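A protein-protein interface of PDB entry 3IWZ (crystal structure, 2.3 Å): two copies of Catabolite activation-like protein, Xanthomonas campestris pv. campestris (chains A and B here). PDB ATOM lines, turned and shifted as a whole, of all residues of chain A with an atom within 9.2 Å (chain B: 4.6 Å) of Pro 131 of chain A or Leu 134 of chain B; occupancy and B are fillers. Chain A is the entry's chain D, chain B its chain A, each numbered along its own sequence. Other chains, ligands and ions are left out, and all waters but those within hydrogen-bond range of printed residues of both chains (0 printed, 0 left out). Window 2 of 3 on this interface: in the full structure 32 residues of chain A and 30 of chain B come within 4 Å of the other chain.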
ATOM      1  N   LEU A  22       7.004  -2.653   1.326  1.00  0.00           N
ATOM      2  CA  LEU A  22       5.801  -3.461   1.661  1.00  0.00           C
ATOM      3  C   LEU A  22       4.882  -3.578   0.448  1.00  0.00           C
ATOM      4  O   LEU A  22       4.699  -2.613  -0.301  1.00  0.00           O
ATOM      5  CB  LEU A  22       5.046  -2.826   2.839  1.00  0.00           C
ATOM      6  CG  LEU A  22       4.258  -1.532   2.617  1.00  0.00           C
ATOM      7  CD1 LEU A  22       3.956  -0.926   3.981  1.00  0.00           C
ATOM      8  CD2 LEU A  22       5.039  -0.545   1.757  1.00  0.00           C
ATOM      9  N   ASP A  23       4.313  -4.771   0.271  1.00  0.00           N
ATOM     10  CA  ASP A  23       3.414  -5.086  -0.846  1.00  0.00           C
ATOM     11  C   ASP A  23       1.964  -4.663  -0.629  1.00  0.00           C
ATOM     12  O   ASP A  23       1.576  -4.265   0.469  1.00  0.00           O
ATOM     13  CB  ASP A  23       3.439  -6.590  -1.122  1.00  0.00           C
ATOM     14  CG  ASP A  23       3.155  -7.412   0.122  1.00  0.00           C
ATOM     15  OD1 ASP A  23       4.088  -7.610   0.932  1.00  0.00           O
ATOM     16  OD2 ASP A  23       2.000  -7.847   0.300  1.00  0.00           O
ATOM     17  N   THR A  26       0.183  -6.865   2.058  1.00  0.00           N
ATOM     18  CA  THR A  26       0.409  -6.529   3.454  1.00  0.00           C
ATOM     19  C   THR A  26      -0.417  -5.283   3.772  1.00  0.00           C
ATOM     20  O   THR A  26      -1.005  -5.166   4.851  1.00  0.00           O
ATOM     21  CB  THR A  26       1.900  -6.230   3.722  1.00  0.00           C
ATOM     22  OG1 THR A  26       2.698  -7.354   3.328  1.00  0.00           O
ATOM     23  CG2 THR A  26       2.126  -5.953   5.196  1.00  0.00           C
ATOM     24  N   PHE A  92       6.043   4.509  19.209  1.00  0.00           N
ATOM     25  CA  PHE A  92       7.432   4.241  19.555  1.00  0.00           C
ATOM     26  C   PHE A  92       7.863   4.904  20.853  1.00  0.00           C
ATOM     27  O   PHE A  92       8.673   4.360  21.594  1.00  0.00           O
ATOM     28  CB  PHE A  92       8.331   4.745  18.433  1.00  0.00           C
ATOM     29  CG  PHE A  92       8.161   4.012  17.147  1.00  0.00           C
ATOM     30  CD1 PHE A  92       8.824   2.812  16.931  1.00  0.00           C
ATOM     31  CD2 PHE A  92       7.354   4.528  16.141  1.00  0.00           C
ATOM     32  CE1 PHE A  92       8.691   2.136  15.727  1.00  0.00           C
ATOM     33  CE2 PHE A  92       7.211   3.857  14.926  1.00  0.00           C
ATOM     34  CZ  PHE A  92       7.879   2.663  14.717  1.00  0.00           C
ATOM     35  N   PHE A 122      -0.199  -7.172  15.922  1.00  0.00           N
ATOM     36  CA  PHE A 122       1.182  -7.535  15.603  1.00  0.00           C
ATOM     37  C   PHE A 122       1.543  -8.848  16.283  1.00  0.00           C
ATOM     38  O   PHE A 122       2.529  -9.495  15.921  1.00  0.00           O
ATOM     39  CB  PHE A 122       2.162  -6.449  16.066  1.00  0.00           C
ATOM     40  CG  PHE A 122       2.385  -5.346  15.062  1.00  0.00           C
ATOM     41  CD1 PHE A 122       3.228  -4.281  15.368  1.00  0.00           C
ATOM     42  CD2 PHE A 122       1.761  -5.367  13.815  1.00  0.00           C
ATOM     43  CE1 PHE A 122       3.449  -3.255  14.452  1.00  0.00           C
ATOM     44  CE2 PHE A 122       1.977  -4.343  12.890  1.00  0.00           C
ATOM     45  CZ  PHE A 122       2.822  -3.284  13.214  1.00  0.00           C
ATOM     46  N   GLN A 123       0.751  -9.227  17.281  1.00  0.00           N
ATOM     47  CA  GLN A 123       0.968 -10.476  17.998  1.00  0.00           C
ATOM     48  C   GLN A 123      -0.050 -11.552  17.597  1.00  0.00           C
ATOM     49  O   GLN A 123      -0.033 -12.662  18.129  1.00  0.00           O
ATOM     50  CB  GLN A 123       0.920 -10.237  19.506  1.00  0.00           C
ATOM     51  CG  GLN A 123       2.123  -9.467  20.028  1.00  0.00           C
ATOM     52  CD  GLN A 123       3.449 -10.154  19.710  1.00  0.00           C
ATOM     53  OE1 GLN A 123       3.787 -10.371  18.547  1.00  0.00           O
ATOM     54  NE2 GLN A 123       4.205 -10.496  20.751  1.00  0.00           N
ATOM     55  N   LEU A 126      -1.475 -10.405  12.345  1.00  0.00           N
ATOM     56  CA  LEU A 126      -0.581  -9.497  11.617  1.00  0.00           C
ATOM     57  C   LEU A 126       0.902  -9.719  11.916  1.00  0.00           C
ATOM     58  O   LEU A 126       1.767  -9.078  11.322  1.00  0.00           O
ATOM     59  CB  LEU A 126      -0.969  -8.035  11.899  1.00  0.00           C
ATOM     60  CG  LEU A 126      -1.902  -7.355  10.883  1.00  0.00           C
ATOM     61  CD1 LEU A 126      -2.973  -8.327  10.406  1.00  0.00           C
ATOM     62  CD2 LEU A 126      -2.523  -6.106  11.516  1.00  0.00           C
ATOM     63  N   SER A 127       1.186 -10.645  12.825  1.00  0.00           N
ATOM     64  CA  SER A 127       2.557 -10.969  13.213  1.00  0.00           C
ATOM     65  C   SER A 127       3.498 -11.138  12.009  1.00  0.00           C
ATOM     66  O   SER A 127       4.628 -10.645  12.027  1.00  0.00           O
ATOM     67  CB  SER A 127       2.559 -12.243  14.072  1.00  0.00           C
ATOM     68  OG  SER A 127       3.819 -12.467  14.683  1.00  0.00           O
ATOM     69  N   PRO A 128       3.048 -11.838  10.951  1.00  0.00           N
ATOM     70  CA  PRO A 128       3.887 -12.045   9.760  1.00  0.00           C
ATOM     71  C   PRO A 128       4.123 -10.760   8.963  1.00  0.00           C
ATOM     72  O   PRO A 128       5.079 -10.653   8.192  1.00  0.00           O
ATOM     73  CB  PRO A 128       3.094 -13.073   8.950  1.00  0.00           C
ATOM     74  CG  PRO A 128       2.290 -13.806  10.001  1.00  0.00           C
ATOM     75  CD  PRO A 128       1.834 -12.671  10.878  1.00  0.00           C
ATOM     76  N   ASP A 129       3.234  -9.793   9.146  1.00  0.00           N
ATOM     77  CA  ASP A 129       3.334  -8.517   8.454  1.00  0.00           C
ATOM     78  C   ASP A 129       4.159  -7.510   9.270  1.00  0.00           C
ATOM     79  O   ASP A 129       4.645  -6.520   8.732  1.00  0.00           O
ATOM     80  CB  ASP A 129       1.925  -7.971   8.198  1.00  0.00           C
ATOM     81  CG  ASP A 129       1.098  -8.878   7.290  1.00  0.00           C
ATOM     82  OD1 ASP A 129      -0.150  -8.823   7.358  1.00  0.00           O
ATOM     83  OD2 ASP A 129       1.694  -9.639   6.500  1.00  0.00           O
ATOM     84  N   ALA A 130       4.318  -7.780  10.564  1.00  0.00           N
ATOM     85  CA  ALA A 130       5.066  -6.900  11.460  1.00  0.00           C
ATOM     86  C   ALA A 130       6.412  -6.471  10.886  1.00  0.00           C
ATOM     87  O   ALA A 130       6.712  -5.282  10.824  1.00  0.00           O
ATOM     88  CB  ALA A 130       5.264  -7.583  12.812  1.00  0.00           C
ATOM     89  N   PRO A 131       7.244  -7.433  10.453  1.00  0.00           N
ATOM     90  CA  PRO A 131       8.550  -7.077   9.888  1.00  0.00           C
ATOM     91  C   PRO A 131       8.461  -6.038   8.766  1.00  0.00           C
ATOM     92  O   PRO A 131       9.170  -5.030   8.796  1.00  0.00           O
ATOM     93  CB  PRO A 131       9.088  -8.418   9.394  1.00  0.00           C
ATOM     94  CG  PRO A 131       8.510  -9.375  10.387  1.00  0.00           C
ATOM     95  CD  PRO A 131       7.081  -8.895  10.508  1.00  0.00           C
ATOM     96  N   ARG A 132       7.600  -6.285   7.782  1.00  0.00           N
ATOM     97  CA  ARG A 132       7.445  -5.349   6.663  1.00  0.00           C
ATOM     98  C   ARG A 132       6.844  -4.015   7.083  1.00  0.00           C
ATOM     99  O   ARG A 132       7.179  -2.978   6.519  1.00  0.00           O
ATOM    100  CB  ARG A 132       6.567  -5.936   5.557  1.00  0.00           C
ATOM    101  CG  ARG A 132       7.319  -6.694   4.481  1.00  0.00           C
ATOM    102  CD  ARG A 132       6.353  -7.181   3.415  1.00  0.00           C
ATOM    103  NE  ARG A 132       5.347  -8.091   3.966  1.00  0.00           N
ATOM    104  CZ  ARG A 132       5.572  -9.370   4.258  1.00  0.00           C
ATOM    105  NH1 ARG A 132       6.771  -9.900   4.048  1.00  0.00           N
ATOM    106  NH2 ARG A 132       4.595 -10.122   4.760  1.00  0.00           N
ATOM    107  N   ILE A 133       5.947  -4.040   8.061  1.00  0.00           N
ATOM    108  CA  ILE A 133       5.323  -2.809   8.518  1.00  0.00           C
ATOM    109  C   ILE A 133       6.385  -1.921   9.176  1.00  0.00           C
ATOM    110  O   ILE A 133       6.635  -0.790   8.744  1.00  0.00           O
ATOM    111  CB  ILE A 133       4.215  -3.083   9.547  1.00  0.00           C
ATOM    112  CG1 ILE A 133       3.202  -4.096   8.997  1.00  0.00           C
ATOM    113  CG2 ILE A 133       3.521  -1.776   9.902  1.00  0.00           C
ATOM    114  CD1 ILE A 133       2.361  -3.601   7.855  1.00  0.00           C
ATOM    115  N   LEU A 134       7.006  -2.447  10.225  1.00  0.00           N
ATOM    116  CA  LEU A 134       8.032  -1.721  10.961  1.00  0.00           C
ATOM    117  C   LEU A 134       9.134  -1.194  10.056  1.00  0.00           C
ATOM    118  O   LEU A 134       9.580  -0.059  10.210  1.00  0.00           O
ATOM    119  CB  LEU A 134       8.629  -2.628  12.030  1.00  0.00           C
ATOM    120  CG  LEU A 134       7.615  -3.048  13.082  1.00  0.00           C
ATOM    121  CD1 LEU A 134       8.199  -4.154  13.949  1.00  0.00           C
ATOM    122  CD2 LEU A 134       7.230  -1.824  13.912  1.00  0.00           C
ATOM    123  N   TYR A 135       9.560  -2.012   9.102  1.00  0.00           N
ATOM    124  CA  TYR A 135      10.610  -1.596   8.183  1.00  0.00           C
ATOM    125  C   TYR A 135      10.127  -0.435   7.318  1.00  0.00           C
ATOM    126  O   TYR A 135      10.869   0.519   7.088  1.00  0.00           O
ATOM    127  CB  TYR A 135      11.036  -2.764   7.293  1.00  0.00           C
ATOM    128  CG  TYR A 135      12.124  -2.407   6.306  1.00  0.00           C
ATOM    129  CD1 TYR A 135      13.439  -2.227   6.723  1.00  0.00           C
ATOM    130  CD2 TYR A 135      11.825  -2.195   4.961  1.00  0.00           C
ATOM    131  CE1 TYR A 135      14.429  -1.838   5.831  1.00  0.00           C
ATOM    132  CE2 TYR A 135      12.810  -1.803   4.057  1.00  0.00           C
ATOM    133  CZ  TYR A 135      14.108  -1.624   4.499  1.00  0.00           C
ATOM    134  OH  TYR A 135      15.074  -1.195   3.619  1.00  0.00           O
ATOM    135  N   ALA A 136       8.893  -0.516   6.825  1.00  0.00           N
ATOM    136  CA  ALA A 136       8.358   0.569   6.004  1.00  0.00           C
ATOM    137  C   ALA A 136       8.355   1.861   6.821  1.00  0.00           C
ATOM    138  O   ALA A 136       8.771   2.910   6.335  1.00  0.00           O
ATOM    139  CB  ALA A 136       6.944   0.249   5.537  1.00  0.00           C
ATOM    140  N   ILE A 137       7.887   1.779   8.066  1.00  0.00           N
ATOM    141  CA  ILE A 137       7.851   2.950   8.929  1.00  0.00           C
ATOM    142  C   ILE A 137       9.281   3.427   9.152  1.00  0.00           C
ATOM    143  O   ILE A 137       9.543   4.627   9.230  1.00  0.00           O
ATOM    144  CB  ILE A 137       7.174   2.626  10.277  1.00  0.00           C
ATOM    145  CG1 ILE A 137       5.687   2.323  10.042  1.00  0.00           C
ATOM    146  CG2 ILE A 137       7.355   3.785  11.252  1.00  0.00           C
ATOM    147  CD1 ILE A 137       4.924   1.958  11.282  1.00  0.00           C
ATOM    148  N   GLY A 138      10.208   2.478   9.238  1.00  0.00           N
ATOM    149  CA  GLY A 138      11.602   2.834   9.415  1.00  0.00           C
ATOM    150  C   GLY A 138      12.076   3.665   8.235  1.00  0.00           C
ATOM    151  O   GLY A 138      12.751   4.687   8.400  1.00  0.00           O
ATOM    152  N   VAL A 139      11.733   3.220   7.031  1.00  0.00           N
ATOM    153  CA  VAL A 139      12.103   3.938   5.813  1.00  0.00           C
ATOM    154  C   VAL A 139      11.576   5.370   5.861  1.00  0.00           C
ATOM    155  O   VAL A 139      12.288   6.327   5.527  1.00  0.00           O
ATOM    156  CB  VAL A 139      11.509   3.254   4.562  1.00  0.00           C
ATOM    157  CG1 VAL A 139      11.631   4.179   3.351  1.00  0.00           C
ATOM    158  CG2 VAL A 139      12.222   1.918   4.310  1.00  0.00           C
ATOM    159  N   LEU A 141      10.628   7.109   8.572  1.00  0.00           N
ATOM    160  CA  LEU A 141      11.236   7.865   9.654  1.00  0.00           C
ATOM    161  C   LEU A 141      12.612   8.334   9.188  1.00  0.00           C
ATOM    162  O   LEU A 141      12.998   9.473   9.434  1.00  0.00           O
ATOM    163  CB  LEU A 141      11.356   7.005  10.924  1.00  0.00           C
ATOM    164  CG  LEU A 141      10.061   6.802  11.746  1.00  0.00           C
ATOM    165  CD1 LEU A 141      10.290   5.823  12.893  1.00  0.00           C
ATOM    166  CD2 LEU A 141       9.588   8.145  12.297  1.00  0.00           C
ATOM    167  N   PHE B  92      17.896   1.770   5.407  1.00  0.00           N
ATOM    168  CA  PHE B  92      16.542   2.165   5.052  1.00  0.00           C
ATOM    169  C   PHE B  92      16.462   2.980   3.758  1.00  0.00           C
ATOM    170  O   PHE B  92      15.481   2.898   3.033  1.00  0.00           O
ATOM    171  CB  PHE B  92      15.952   2.985   6.199  1.00  0.00           C
ATOM    172  CG  PHE B  92      15.794   2.214   7.486  1.00  0.00           C
ATOM    173  CD1 PHE B  92      14.667   1.416   7.703  1.00  0.00           C
ATOM    174  CD2 PHE B  92      16.748   2.314   8.495  1.00  0.00           C
ATOM    175  CE1 PHE B  92      14.495   0.728   8.899  1.00  0.00           C
ATOM    176  CE2 PHE B  92      16.587   1.626   9.705  1.00  0.00           C
ATOM    177  CZ  PHE B  92      15.457   0.836   9.909  1.00  0.00           C
ATOM    178  N   PHE B 122      18.411 -11.398   8.643  1.00  0.00           N
ATOM    179  CA  PHE B 122      16.984 -11.183   8.882  1.00  0.00           C
ATOM    180  C   PHE B 122      16.118 -12.237   8.174  1.00  0.00           C
ATOM    181  O   PHE B 122      15.055 -12.607   8.670  1.00  0.00           O
ATOM    182  CB  PHE B 122      16.552  -9.791   8.402  1.00  0.00           C
ATOM    183  CG  PHE B 122      16.806  -8.679   9.395  1.00  0.00           C
ATOM    184  CD1 PHE B 122      16.399  -7.377   9.105  1.00  0.00           C
ATOM    185  CD2 PHE B 122      17.446  -8.924  10.607  1.00  0.00           C
ATOM    186  CE1 PHE B 122      16.641  -6.334   9.999  1.00  0.00           C
ATOM    187  CE2 PHE B 122      17.690  -7.893  11.502  1.00  0.00           C
ATOM    188  CZ  PHE B 122      17.281  -6.595  11.201  1.00  0.00           C
ATOM    189  N   ALA B 130      14.136 -10.005  13.935  1.00  0.00           N
ATOM    190  CA  ALA B 130      13.931  -8.937  12.973  1.00  0.00           C
ATOM    191  C   ALA B 130      12.966  -7.887  13.515  1.00  0.00           C
ATOM    192  O   ALA B 130      13.291  -6.695  13.565  1.00  0.00           O
ATOM    193  CB  ALA B 130      13.411  -9.507  11.648  1.00  0.00           C
ATOM    194  N   PRO B 131      11.768  -8.317  13.938  1.00  0.00           N
ATOM    195  CA  PRO B 131      10.791  -7.368  14.470  1.00  0.00           C
ATOM    196  C   PRO B 131      11.300  -6.538  15.646  1.00  0.00           C
ATOM    197  O   PRO B 131      10.972  -5.362  15.748  1.00  0.00           O
ATOM    198  CB  PRO B 131       9.621  -8.269  14.862  1.00  0.00           C
ATOM    199  CG  PRO B 131       9.718  -9.382  13.869  1.00  0.00           C
ATOM    200  CD  PRO B 131      11.193  -9.671  13.874  1.00  0.00           C
ATOM    201  N   ARG B 132      12.092  -7.148  16.530  1.00  0.00           N
ATOM    202  CA  ARG B 132      12.608  -6.438  17.706  1.00  0.00           C
ATOM    203  C   ARG B 132      13.701  -5.434  17.363  1.00  0.00           C
ATOM    204  O   ARG B 132      13.708  -4.309  17.859  1.00  0.00           O
ATOM    205  CB  ARG B 132      13.128  -7.425  18.760  1.00  0.00           C
ATOM    206  CG  ARG B 132      12.035  -8.017  19.649  1.00  0.00           C
ATOM    207  CD  ARG B 132      12.627  -8.778  20.837  1.00  0.00           C
ATOM    208  NE  ARG B 132      13.189 -10.068  20.440  1.00  0.00           N
ATOM    209  CZ  ARG B 132      12.463 -11.146  20.153  1.00  0.00           C
ATOM    210  NH1 ARG B 132      11.135 -11.093  20.219  1.00  0.00           N
ATOM    211  NH2 ARG B 132      13.064 -12.278  19.805  1.00  0.00           N
ATOM    212  N   ILE B 133      14.628  -5.852  16.516  1.00  0.00           N
ATOM    213  CA  ILE B 133      15.696  -4.971  16.106  1.00  0.00           C
ATOM    214  C   ILE B 133      15.090  -3.825  15.306  1.00  0.00           C
ATOM    215  O   ILE B 133      15.465  -2.670  15.493  1.00  0.00           O
ATOM    216  CB  ILE B 133      16.734  -5.731  15.272  1.00  0.00           C
ATOM    217  CG1 ILE B 133      17.520  -6.680  16.191  1.00  0.00           C
ATOM    218  CG2 ILE B 133      17.667  -4.768  14.608  1.00  0.00           C
ATOM    219  CD1 ILE B 133      18.501  -7.586  15.483  1.00  0.00           C
ATOM    220  N   LEU B 134      14.126  -4.137  14.445  1.00  0.00           N
ATOM    221  CA  LEU B 134      13.480  -3.109  13.642  1.00  0.00           C
ATOM    222  C   LEU B 134      12.708  -2.100  14.485  1.00  0.00           C
ATOM    223  O   LEU B 134      12.794  -0.899  14.256  1.00  0.00           O
ATOM    224  CB  LEU B 134      12.560  -3.747  12.600  1.00  0.00           C
ATOM    225  CG  LEU B 134      13.313  -4.407  11.432  1.00  0.00           C
ATOM    226  CD1 LEU B 134      12.342  -5.103  10.492  1.00  0.00           C
ATOM    227  CD2 LEU B 134      14.102  -3.349  10.691  1.00  0.00           C
ATOM    228  N   TYR B 135      11.961  -2.590  15.468  1.00  0.00           N
ATOM    229  CA  TYR B 135      11.183  -1.716  16.341  1.00  0.00           C
ATOM    230  C   TYR B 135      12.128  -0.830  17.160  1.00  0.00           C
ATOM    231  O   TYR B 135      11.890   0.367  17.336  1.00  0.00           O
ATOM    232  CB  TYR B 135      10.316  -2.540  17.303  1.00  0.00           C
ATOM    233  CG  TYR B 135       9.512  -1.687  18.254  1.00  0.00           C
ATOM    234  CD1 TYR B 135       8.409  -0.968  17.801  1.00  0.00           C
ATOM    235  CD2 TYR B 135       9.883  -1.551  19.593  1.00  0.00           C
ATOM    236  CE1 TYR B 135       7.694  -0.133  18.645  1.00  0.00           C
ATOM    237  CE2 TYR B 135       9.173  -0.707  20.457  1.00  0.00           C
ATOM    238  CZ  TYR B 135       8.077  -0.001  19.968  1.00  0.00           C
ATOM    239  OH  TYR B 135       7.361   0.838  20.778  1.00  0.00           O
ATOM    240  N   ALA B 136      13.210  -1.423  17.658  1.00  0.00           N
ATOM    241  CA  ALA B 136      14.155  -0.662  18.463  1.00  0.00           C
ATOM    242  C   ALA B 136      14.777   0.480  17.650  1.00  0.00           C
ATOM    243  O   ALA B 136      14.910   1.589  18.153  1.00  0.00           O
ATOM    244  CB  ALA B 136      15.236  -1.588  19.021  1.00  0.00           C
ATOM    245  N   ILE B 137      15.158   0.204  16.405  1.00  0.00           N
ATOM    246  CA  ILE B 137      15.742   1.233  15.549  1.00  0.00           C
ATOM    247  C   ILE B 137      14.679   2.318  15.313  1.00  0.00           C
ATOM    248  O   ILE B 137      14.988   3.507  15.184  1.00  0.00           O
ATOM    249  CB  ILE B 137      16.207   0.644  14.183  1.00  0.00           C
ATOM    250  CG1 ILE B 137      17.468  -0.210  14.384  1.00  0.00           C
ATOM    251  CG2 ILE B 137      16.476   1.766  13.188  1.00  0.00           C
ATOM    252  CD1 ILE B 137      17.993  -0.845  13.100  1.00  0.00           C
ATOM    253  N   GLY B 138      13.422   1.891  15.249  1.00  0.00           N
ATOM    254  CA  GLY B 138      12.341   2.835  15.056  1.00  0.00           C
ATOM    255  C   GLY B 138      12.214   3.747  16.269  1.00  0.00           C
ATOM    256  O   GLY B 138      11.866   4.920  16.139  1.00  0.00           O
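CD1 of Phe 92 of chain A touches CE1 of Tyr 135 of chain B (3.6 Å).
Gly 138 of chain B touches Phe 92 of chain A (C to CD1, 3.6 Å).
Pro 131 of chain B touches Pro 131 of chain A (CG to CG, 3.7 Å).
Pro 131 of chain A touches Leu 134 of chain B.
CD1 of Leu 134 of chain A touches O of Pro 131 of chain B (3.5 Å).
CD1 of Phe 92 of chain B touches CE1 of Tyr 135 of chain A (3.8 Å).
Gly 138 of chain A touches Phe 92 of chain B (C to CD1, 3.5 Å).
N of Val 139 of chain A touches CD1 of Phe 92 of chain B, at 3.5 Å.
Gly 138 of chain B touches Leu 141 of chain A.
Printed residues of chain B within 4 Å of Leu 134 of chain A: Pro 131.
Of the printed residues of chain B, Tyr 135 of chain A touches Phe 92 (3.8 Å).
Of the printed residues of chain B, Val 139 of chain A touches Phe 92 (3.5 Å).
Of the printed residues of chain B, Leu 141 of chain A touches Gly 138.
Printed residues of chain A within 4 Å of Leu 134 of chain B: Pro 131 (3.6 Å).
Printed residues of chain A within 4 Å of Tyr 135 of chain B: Phe 92.
No residue of chain A comes within 4 Å of Ile 137 of chain B.
The nearest printed residue of chain B that does not touch Pro 131 of chain A is Ala 130 of chain B (5.0 Å).
Of the 11 printed residues of chain B, 5 touch a printed residue of chain A.
Along chain B the printed residues that touch a printed residue of chain A span positions 92 to 138.
Hydrophobic or aromatic side chains of chain A within 4 Å of the printed part of chain B: Phe 92, Pro 131, Leu 134, Tyr 135, Val 139 and Leu 141.
Among the printed residues, 9 pairs touch across the chains.
Phe 92 of chain A touches Tyr 135 of chain B, and with the chains exchanged Tyr 135 of chain A touches Phe 92 of chain B.
Phe 92 of chain A touches Gly 138 of chain B, and with the chains exchanged Gly 138 of chain A touches Phe 92 of chain B.
Pro 131 of chain A touches its own counterpart, Pro 131 of chain B.
Pro 131 of chain A touches Leu 134 of chain B, and with the chains exchanged Leu 134 of chain A touches Pro 131 of chain B.
Positions printed for both chains: 92, 122, 130, 131, 132, 133, 134, 135, 136, 137 and 138.
Of the 9 pairs that touch across the chains among the printed residues, 7 have their exchanged pair printed and touching as well.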
